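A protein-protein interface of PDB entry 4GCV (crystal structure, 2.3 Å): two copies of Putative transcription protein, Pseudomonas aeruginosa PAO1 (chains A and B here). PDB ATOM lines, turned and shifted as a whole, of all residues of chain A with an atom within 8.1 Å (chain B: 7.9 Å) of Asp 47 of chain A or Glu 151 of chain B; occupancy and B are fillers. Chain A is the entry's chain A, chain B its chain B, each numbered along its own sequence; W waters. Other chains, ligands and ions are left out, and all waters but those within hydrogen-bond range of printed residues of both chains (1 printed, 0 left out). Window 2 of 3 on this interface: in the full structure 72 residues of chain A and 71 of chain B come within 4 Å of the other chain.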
ATOM      1  N   TRP A  23     -21.168 -33.632 -11.926  1.00  0.00           N
ATOM      2  CA  TRP A  23     -22.164 -32.582 -12.193  1.00  0.00           C
ATOM      3  C   TRP A  23     -23.274 -33.009 -13.180  1.00  0.00           C
ATOM      4  O   TRP A  23     -24.477 -32.903 -12.859  1.00  0.00           O
ATOM      5  CB  TRP A  23     -21.470 -31.310 -12.649  1.00  0.00           C
ATOM      6  CG  TRP A  23     -22.341 -30.161 -13.055  1.00  0.00           C
ATOM      7  CD1 TRP A  23     -22.367 -29.561 -14.281  1.00  0.00           C
ATOM      8  CD2 TRP A  23     -23.255 -29.428 -12.239  1.00  0.00           C
ATOM      9  NE1 TRP A  23     -23.247 -28.514 -14.282  1.00  0.00           N
ATOM     10  CE2 TRP A  23     -23.821 -28.426 -13.043  1.00  0.00           C
ATOM     11  CE3 TRP A  23     -23.690 -29.553 -10.917  1.00  0.00           C
ATOM     12  CZ2 TRP A  23     -24.791 -27.538 -12.567  1.00  0.00           C
ATOM     13  CZ3 TRP A  23     -24.651 -28.680 -10.443  1.00  0.00           C
ATOM     14  CH2 TRP A  23     -25.190 -27.678 -11.266  1.00  0.00           C
ATOM     15  N   TRP A  24     -22.877 -33.423 -14.381  1.00  0.00           N
ATOM     16  CA  TRP A  24     -23.827 -33.880 -15.376  1.00  0.00           C
ATOM     17  C   TRP A  24     -24.593 -35.123 -14.902  1.00  0.00           C
ATOM     18  O   TRP A  24     -25.778 -35.218 -15.193  1.00  0.00           O
ATOM     19  CB  TRP A  24     -23.145 -34.161 -16.727  1.00  0.00           C
ATOM     20  CG  TRP A  24     -22.565 -32.918 -17.286  1.00  0.00           C
ATOM     21  CD1 TRP A  24     -21.252 -32.658 -17.526  1.00  0.00           C
ATOM     22  CD2 TRP A  24     -23.285 -31.733 -17.627  1.00  0.00           C
ATOM     23  NE1 TRP A  24     -21.110 -31.381 -18.002  1.00  0.00           N
ATOM     24  CE2 TRP A  24     -22.350 -30.797 -18.074  1.00  0.00           C
ATOM     25  CE3 TRP A  24     -24.643 -31.378 -17.591  1.00  0.00           C
ATOM     26  CZ2 TRP A  24     -22.719 -29.526 -18.484  1.00  0.00           C
ATOM     27  CZ3 TRP A  24     -25.012 -30.151 -18.000  1.00  0.00           C
ATOM     28  CH2 TRP A  24     -24.060 -29.216 -18.434  1.00  0.00           C
ATOM     29  N   LEU A  27     -27.332 -33.851 -12.665  1.00  0.00           N
ATOM     30  CA  LEU A  27     -28.384 -33.180 -13.430  1.00  0.00           C
ATOM     31  C   LEU A  27     -29.206 -34.181 -14.243  1.00  0.00           C
ATOM     32  O   LEU A  27     -30.412 -34.115 -14.237  1.00  0.00           O
ATOM     33  CB  LEU A  27     -27.820 -32.064 -14.332  1.00  0.00           C
ATOM     34  CG  LEU A  27     -27.136 -30.860 -13.660  1.00  0.00           C
ATOM     35  CD1 LEU A  27     -26.657 -29.806 -14.707  1.00  0.00           C
ATOM     36  CD2 LEU A  27     -27.993 -30.210 -12.630  1.00  0.00           C
ATOM     37  N   ASP A  31     -33.292 -35.371 -13.612  1.00  0.00           N
ATOM     38  CA  ASP A  31     -34.270 -35.310 -14.692  1.00  0.00           C
ATOM     39  C   ASP A  31     -34.966 -36.641 -14.951  1.00  0.00           C
ATOM     40  O   ASP A  31     -36.161 -36.671 -15.219  1.00  0.00           O
ATOM     41  CB  ASP A  31     -33.637 -34.804 -15.994  1.00  0.00           C
ATOM     42  CG  ASP A  31     -33.575 -33.290 -16.056  1.00  0.00           C
ATOM     43  OD1 ASP A  31     -33.996 -32.649 -15.078  1.00  0.00           O
ATOM     44  OD2 ASP A  31     -33.116 -32.740 -17.083  1.00  0.00           O
ATOM     45  N   ASP A  40     -33.563 -35.950 -26.690  1.00  0.00           N
ATOM     46  CA  ASP A  40     -33.754 -34.519 -26.911  1.00  0.00           C
ATOM     47  C   ASP A  40     -34.387 -33.802 -25.702  1.00  0.00           C
ATOM     48  O   ASP A  40     -34.132 -32.614 -25.505  1.00  0.00           O
ATOM     49  CB  ASP A  40     -34.511 -34.220 -28.225  1.00  0.00           C
ATOM     50  CG  ASP A  40     -33.623 -34.350 -29.480  1.00  0.00           C
ATOM     51  OD1 ASP A  40     -32.393 -34.542 -29.357  1.00  0.00           O
ATOM     52  OD2 ASP A  40     -34.164 -34.252 -30.608  1.00  0.00           O
ATOM     53  N   GLU A  41     -35.171 -34.523 -24.885  1.00  0.00           N
ATOM     54  CA  GLU A  41     -35.700 -33.961 -23.636  1.00  0.00           C
ATOM     55  C   GLU A  41     -34.578 -33.529 -22.700  1.00  0.00           C
ATOM     56  O   GLU A  41     -34.542 -32.389 -22.243  1.00  0.00           O
ATOM     57  CB  GLU A  41     -36.598 -34.963 -22.913  1.00  0.00           C
ATOM     58  CG  GLU A  41     -37.961 -35.140 -23.575  1.00  0.00           C
ATOM     59  CD  GLU A  41     -38.831 -36.089 -22.796  1.00  0.00           C
ATOM     60  OE1 GLU A  41     -38.298 -37.023 -22.148  1.00  0.00           O
ATOM     61  OE2 GLU A  41     -40.059 -35.892 -22.830  1.00  0.00           O
ATOM     62  N   PHE A  42     -33.662 -34.452 -22.421  1.00  0.00           N
ATOM     63  CA  PHE A  42     -32.478 -34.147 -21.649  1.00  0.00           C
ATOM     64  C   PHE A  42     -31.661 -33.054 -22.333  1.00  0.00           C
ATOM     65  O   PHE A  42     -31.110 -32.186 -21.678  1.00  0.00           O
ATOM     66  CB  PHE A  42     -31.603 -35.389 -21.506  1.00  0.00           C
ATOM     67  CG  PHE A  42     -32.205 -36.467 -20.669  1.00  0.00           C
ATOM     68  CD1 PHE A  42     -32.259 -36.349 -19.277  1.00  0.00           C
ATOM     69  CD2 PHE A  42     -32.665 -37.631 -21.251  1.00  0.00           C
ATOM     70  CE1 PHE A  42     -32.797 -37.379 -18.503  1.00  0.00           C
ATOM     71  CE2 PHE A  42     -33.196 -38.640 -20.489  1.00  0.00           C
ATOM     72  CZ  PHE A  42     -33.284 -38.523 -19.124  1.00  0.00           C
ATOM     73  N   SER A  43     -31.560 -33.129 -23.652  1.00  0.00           N
ATOM     74  CA  SER A  43     -30.749 -32.185 -24.375  1.00  0.00           C
ATOM     75  C   SER A  43     -31.264 -30.763 -24.201  1.00  0.00           C
ATOM     76  O   SER A  43     -30.493 -29.876 -23.906  1.00  0.00           O
ATOM     77  CB  SER A  43     -30.627 -32.560 -25.848  1.00  0.00           C
ATOM     78  OG  SER A  43     -29.597 -31.764 -26.415  1.00  0.00           O
ATOM     79  N   ARG A  44     -32.573 -30.561 -24.319  1.00  0.00           N
ATOM     80  CA  ARG A  44     -33.150 -29.216 -24.202  1.00  0.00           C
ATOM     81  C   ARG A  44     -33.269 -28.755 -22.762  1.00  0.00           C
ATOM     82  O   ARG A  44     -33.043 -27.588 -22.468  1.00  0.00           O
ATOM     83  CB  ARG A  44     -34.551 -29.125 -24.837  1.00  0.00           C
ATOM     84  CG  ARG A  44     -34.750 -29.801 -26.198  1.00  0.00           C
ATOM     85  CD  ARG A  44     -33.920 -29.229 -27.325  1.00  0.00           C
ATOM     86  NE  ARG A  44     -34.559 -29.497 -28.628  1.00  0.00           N
ATOM     87  CZ  ARG A  44     -34.089 -30.341 -29.552  1.00  0.00           C
ATOM     88  NH1 ARG A  44     -32.931 -31.011 -29.348  1.00  0.00           N
ATOM     89  NH2 ARG A  44     -34.768 -30.505 -30.690  1.00  0.00           N
ATOM     90  N   SER A  45     -33.658 -29.662 -21.871  1.00  0.00           N
ATOM     91  CA  SER A  45     -33.884 -29.284 -20.499  1.00  0.00           C
ATOM     92  C   SER A  45     -32.585 -28.933 -19.827  1.00  0.00           C
ATOM     93  O   SER A  45     -32.514 -27.955 -19.085  1.00  0.00           O
ATOM     94  CB  SER A  45     -34.622 -30.372 -19.751  1.00  0.00           C
ATOM     95  OG  SER A  45     -33.996 -30.641 -18.483  1.00  0.00           O
ATOM     96  N   LEU A  46     -31.540 -29.690 -20.134  1.00  0.00           N
ATOM     97  CA  LEU A  46     -30.235 -29.489 -19.509  1.00  0.00           C
ATOM     98  C   LEU A  46     -29.317 -28.546 -20.294  1.00  0.00           C
ATOM     99  O   LEU A  46     -28.320 -28.047 -19.770  1.00  0.00           O
ATOM    100  CB  LEU A  46     -29.592 -30.860 -19.306  1.00  0.00           C
ATOM    101  CG  LEU A  46     -29.767 -31.555 -17.949  1.00  0.00           C
ATOM    102  CD1 LEU A  46     -30.789 -30.869 -17.038  1.00  0.00           C
ATOM    103  CD2 LEU A  46     -30.046 -32.996 -18.096  1.00  0.00           C
ATOM    104  N   ASP A  47     -29.664 -28.267 -21.549  1.00  0.00           N
ATOM    105  CA  ASP A  47     -28.814 -27.464 -22.421  1.00  0.00           C
ATOM    106  C   ASP A  47     -27.400 -28.006 -22.444  1.00  0.00           C
ATOM    107  O   ASP A  47     -26.431 -27.312 -22.104  1.00  0.00           O
ATOM    108  CB  ASP A  47     -28.816 -25.982 -22.036  1.00  0.00           C
ATOM    109  CG  ASP A  47     -28.095 -25.105 -23.071  1.00  0.00           C
ATOM    110  OD1 ASP A  47     -28.184 -25.375 -24.299  1.00  0.00           O
ATOM    111  OD2 ASP A  47     -27.425 -24.140 -22.670  1.00  0.00           O
ATOM    112  N   ILE A  48     -27.304 -29.250 -22.875  1.00  0.00           N
ATOM    113  CA  ILE A  48     -26.064 -29.997 -22.919  1.00  0.00           C
ATOM    114  C   ILE A  48     -25.860 -30.445 -24.385  1.00  0.00           C
ATOM    115  O   ILE A  48     -26.823 -30.845 -25.072  1.00  0.00           O
ATOM    116  CB  ILE A  48     -26.146 -31.192 -21.908  1.00  0.00           C
ATOM    117  CG1 ILE A  48     -24.891 -32.049 -21.952  1.00  0.00           C
ATOM    118  CG2 ILE A  48     -27.372 -32.049 -22.159  1.00  0.00           C
ATOM    119  CD1 ILE A  48     -24.775 -33.049 -20.786  1.00  0.00           C
ATOM    120  N   ALA A  49     -24.621 -30.369 -24.856  1.00  0.00           N
ATOM    121  CA  ALA A  49     -24.269 -30.793 -26.180  1.00  0.00           C
ATOM    122  C   ALA A  49     -24.356 -32.301 -26.307  1.00  0.00           C
ATOM    123  O   ALA A  49     -24.128 -33.021 -25.338  1.00  0.00           O
ATOM    124  CB  ALA A  49     -22.871 -30.303 -26.529  1.00  0.00           C
ATOM    125  N   PRO A  50     -24.664 -32.792 -27.501  1.00  0.00           N
ATOM    126  CA  PRO A  50     -24.978 -34.236 -27.684  1.00  0.00           C
ATOM    127  C   PRO A  50     -23.867 -35.279 -27.417  1.00  0.00           C
ATOM    128  O   PRO A  50     -24.175 -36.349 -26.881  1.00  0.00           O
ATOM    129  CB  PRO A  50     -25.483 -34.327 -29.120  1.00  0.00           C
ATOM    130  CG  PRO A  50     -25.740 -32.857 -29.580  1.00  0.00           C
ATOM    131  CD  PRO A  50     -24.974 -31.957 -28.679  1.00  0.00           C
ATOM    132  N   LEU A  53     -23.625 -35.628 -23.641  1.00  0.00           N
ATOM    133  CA  LEU A  53     -24.834 -36.282 -23.127  1.00  0.00           C
ATOM    134  C   LEU A  53     -24.801 -37.782 -23.382  1.00  0.00           C
ATOM    135  O   LEU A  53     -25.190 -38.553 -22.513  1.00  0.00           O
ATOM    136  CB  LEU A  53     -26.112 -35.675 -23.735  1.00  0.00           C
ATOM    137  CG  LEU A  53     -27.480 -36.230 -23.330  1.00  0.00           C
ATOM    138  CD1 LEU A  53     -27.661 -36.209 -21.804  1.00  0.00           C
ATOM    139  CD2 LEU A  53     -28.547 -35.399 -23.988  1.00  0.00           C
ATOM    140  N   ALA B 148     -28.486 -18.411  -8.196  1.00  0.00           N
ATOM    141  CA  ALA B 148     -28.634 -19.062  -9.526  1.00  0.00           C
ATOM    142  C   ALA B 148     -28.843 -18.142 -10.728  1.00  0.00           C
ATOM    143  O   ALA B 148     -29.771 -17.307 -10.749  1.00  0.00           O
ATOM    144  CB  ALA B 148     -29.720 -20.143  -9.501  1.00  0.00           C
ATOM    145  N   SER B 149     -27.977 -18.314 -11.727  1.00  0.00           N
ATOM    146  CA  SER B 149     -28.170 -17.715 -13.076  1.00  0.00           C
ATOM    147  C   SER B 149     -29.399 -18.303 -13.767  1.00  0.00           C
ATOM    148  O   SER B 149     -29.868 -19.402 -13.389  1.00  0.00           O
ATOM    149  CB  SER B 149     -26.947 -17.989 -13.968  1.00  0.00           C
ATOM    150  OG  SER B 149     -26.766 -19.393 -14.168  1.00  0.00           O
ATOM    151  N   GLU B 150     -29.866 -17.592 -14.795  1.00  0.00           N
ATOM    152  CA  GLU B 150     -30.910 -18.034 -15.747  1.00  0.00           C
ATOM    153  C   GLU B 150     -30.673 -19.485 -16.219  1.00  0.00           C
ATOM    154  O   GLU B 150     -31.591 -20.303 -16.189  1.00  0.00           O
ATOM    155  CB  GLU B 150     -30.970 -17.062 -16.944  1.00  0.00           C
ATOM    156  CG  GLU B 150     -32.303 -17.053 -17.760  1.00  0.00           C
ATOM    157  CD  GLU B 150     -32.399 -15.924 -18.834  1.00  0.00           C
ATOM    158  OE1 GLU B 150     -31.419 -15.683 -19.589  1.00  0.00           O
ATOM    159  OE2 GLU B 150     -33.475 -15.277 -18.938  1.00  0.00           O
ATOM    160  N   GLU B 151     -29.435 -19.794 -16.611  1.00  0.00           N
ATOM    161  CA  GLU B 151     -29.058 -21.115 -17.075  1.00  0.00           C
ATOM    162  C   GLU B 151     -29.289 -22.153 -15.982  1.00  0.00           C
ATOM    163  O   GLU B 151     -29.825 -23.236 -16.244  1.00  0.00           O
ATOM    164  CB  GLU B 151     -27.582 -21.142 -17.472  1.00  0.00           C
ATOM    165  CG  GLU B 151     -27.305 -21.008 -18.947  1.00  0.00           C
ATOM    166  CD  GLU B 151     -27.564 -22.298 -19.719  1.00  0.00           C
ATOM    167  OE1 GLU B 151     -26.878 -23.316 -19.435  1.00  0.00           O
ATOM    168  OE2 GLU B 151     -28.449 -22.288 -20.605  1.00  0.00           O
ATOM    169  N   MET B 152     -28.869 -21.827 -14.760  1.00  0.00           N
ATOM    170  CA  MET B 152     -29.035 -22.754 -13.655  1.00  0.00           C
ATOM    171  C   MET B 152     -30.502 -23.073 -13.395  1.00  0.00           C
ATOM    172  O   MET B 152     -30.853 -24.234 -13.200  1.00  0.00           O
ATOM    173  CB  MET B 152     -28.345 -22.239 -12.384  1.00  0.00           C
ATOM    174  CG  MET B 152     -28.426 -23.216 -11.259  1.00  0.00           C
ATOM    175  SD  MET B 152     -27.372 -24.806 -11.708  1.00  0.00           S
ATOM    176  CE  MET B 152     -25.573 -24.133 -11.270  1.00  0.00           C
ATOM    177  N   ARG B 153     -31.337 -22.036 -13.397  1.00  0.00           N
ATOM    178  CA  ARG B 153     -32.791 -22.138 -13.204  1.00  0.00           C
ATOM    179  C   ARG B 153     -33.442 -23.115 -14.187  1.00  0.00           C
ATOM    180  O   ARG B 153     -34.309 -23.908 -13.811  1.00  0.00           O
ATOM    181  CB  ARG B 153     -33.436 -20.750 -13.374  1.00  0.00           C
ATOM    182  CG  ARG B 153     -32.947 -19.672 -12.401  1.00  0.00           C
ATOM    183  CD  ARG B 153     -34.023 -19.288 -11.402  1.00  0.00           C
ATOM    184  NE  ARG B 153     -34.566 -17.951 -11.637  1.00  0.00           N
ATOM    185  CZ  ARG B 153     -35.636 -17.673 -12.398  1.00  0.00           C
ATOM    186  NH1 ARG B 153     -36.308 -18.645 -13.029  1.00  0.00           N
ATOM    187  NH2 ARG B 153     -36.042 -16.408 -12.538  1.00  0.00           N
ATOM    188  N   GLN B 154     -33.008 -23.033 -15.445  1.00  0.00           N
ATOM    189  CA  GLN B 154     -33.481 -23.887 -16.529  1.00  0.00           C
ATOM    190  C   GLN B 154     -33.072 -25.327 -16.295  1.00  0.00           C
ATOM    191  O   GLN B 154     -33.847 -26.244 -16.552  1.00  0.00           O
ATOM    192  CB  GLN B 154     -32.906 -23.433 -17.877  1.00  0.00           C
ATOM    193  CG  GLN B 154     -33.638 -24.005 -19.108  1.00  0.00           C
ATOM    194  CD  GLN B 154     -32.681 -24.452 -20.225  1.00  0.00           C
ATOM    195  OE1 GLN B 154     -31.773 -25.260 -19.993  1.00  0.00           O
ATOM    196  NE2 GLN B 154     -32.889 -23.936 -21.432  1.00  0.00           N
ATOM    197  N   ARG B 155     -31.850 -25.526 -15.818  1.00  0.00           N
ATOM    198  CA  ARG B 155     -31.362 -26.876 -15.558  1.00  0.00           C
ATOM    199  C   ARG B 155     -32.088 -27.563 -14.402  1.00  0.00           C
ATOM    200  O   ARG B 155     -32.138 -28.807 -14.357  1.00  0.00           O
ATOM    201  CB  ARG B 155     -29.851 -26.895 -15.374  1.00  0.00           C
ATOM    202  CG  ARG B 155     -29.163 -26.536 -16.641  1.00  0.00           C
ATOM    203  CD  ARG B 155     -27.651 -26.372 -16.515  1.00  0.00           C
ATOM    204  NE  ARG B 155     -27.120 -26.534 -17.854  1.00  0.00           N
ATOM    205  CZ  ARG B 155     -26.042 -25.944 -18.354  1.00  0.00           C
ATOM    206  NH1 ARG B 155     -25.310 -25.125 -17.622  1.00  0.00           N
ATOM    207  NH2 ARG B 155     -25.700 -26.199 -19.613  1.00  0.00           N
ATOM    208  N   LEU B 156     -32.719 -26.762 -13.545  1.00  0.00           N
ATOM    209  CA  LEU B 156     -33.359 -27.244 -12.324  1.00  0.00           C
ATOM    210  C   LEU B 156     -34.877 -27.053 -12.318  1.00  0.00           C
ATOM    211  O   LEU B 156     -35.483 -26.889 -13.402  1.00  0.00           O
ATOM    212  CB  LEU B 156     -32.725 -26.569 -11.102  1.00  0.00           C
ATOM    213  CG  LEU B 156     -31.246 -26.894 -10.862  1.00  0.00           C
ATOM    214  CD1 LEU B 156     -30.703 -26.155  -9.613  1.00  0.00           C
ATOM    215  CD2 LEU B 156     -30.996 -28.417 -10.786  1.00  0.00           C
HETATM  216  O   HOH W   1     -31.382 -31.258 -13.196  1.00  0.00           O
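CH2 of Trp 23 of chain A touches CE of Met 152 of chain B, at 3.6 Å. Trp 24 of chain A touches Arg 155 of chain B. Leu 27 of chain A touches Leu 156 of chain B. OE1 of Gln 154 of chain B touches O of Arg 44 of chain A, 3.6 Å away. Arg 155 of chain B touches Ser 45 of chain A (CA to O, 3.9 Å). OE1 of Gln 154 of chain B touches CB of Asp 47 of chain A (3.7 Å).
OE1 of Gln 154 of chain B lies close to O of Ser 45 of chain A (2.9 Å). NE of Arg 155 of chain B sits at hydrogen-bond distance from O of Leu 46 of chain A, at 2.7 Å. NH2 of Arg 155 of chain B lies within hydrogen-bond range of O of Asp 47 of chain A (2.8 Å). The side-chain carboxylate (OE2) of Glu 151 of chain B lies close to the side-chain carboxylate (OD2) of Asp 47 of chain A (3.0 Å).
Water W1 bridges O of Arg 155 of chain B (2.8 Å) and O of Leu 27 of chain A (3.2 Å).
Printed residues of chain B within 4 Å of Asp 47 of chain A: Glu 151 (3.0 Å), Gln 154 (3.7 Å) and Arg 155 (2.8 Å). Glu 151 of chain B touches just one residue of chain A: Asp 47 (3.0 Å). Printed residues of chain B within 4 Å of Leu 46 of chain A: Arg 155. Printed residues of chain B within 4 Å of Leu 27 of chain A: Leu 156 (3.95 Å). Of the printed residues of chain B, Trp 23 of chain A touches Met 152 (3.6 Å). Of the printed residues of chain A, Met 152 of chain B touches Trp 23. Printed residues of chain B within 4 Å of Arg 44 of chain A: Gln 154 (3.6 Å). Pro 50 of chain A touches none of the printed residues of chain B. Ile 48 of chain A touches none of the printed residues of chain B. The nearest printed residue of chain B that does not touch Trp 23 of chain A is Arg 155 of chain B (5.0 Å).
Of the 16 printed residues of chain A, 7 touch a printed residue of chain B. Among the printed residues, 10 pairs touch across the chains. Among the printed residues, no Asp or Glu carboxylate lies within 4 Å of a Lys or Arg side-chain nitrogen of the other chain.
OG of Ser 45 of chain A sits at hydrogen-bond distance from OD2 of Asp 31 of chain A (2.7 Å). OD1 of Asp 40 of chain A is in salt-bridge range of NH1 of Arg 44 of chain A (3.6 Å). The backbone NH (N) of Met 152 of chain B sits at hydrogen-bond distance from the side-chain hydroxyl (OG) of Ser 149 of chain B (3.3 Å). The side-chain carboxylate of Glu 151 of chain B lies within salt-bridge range of the guanidinium group of Arg 155 of chain B (3.0 Å).
No position is printed for both chains.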
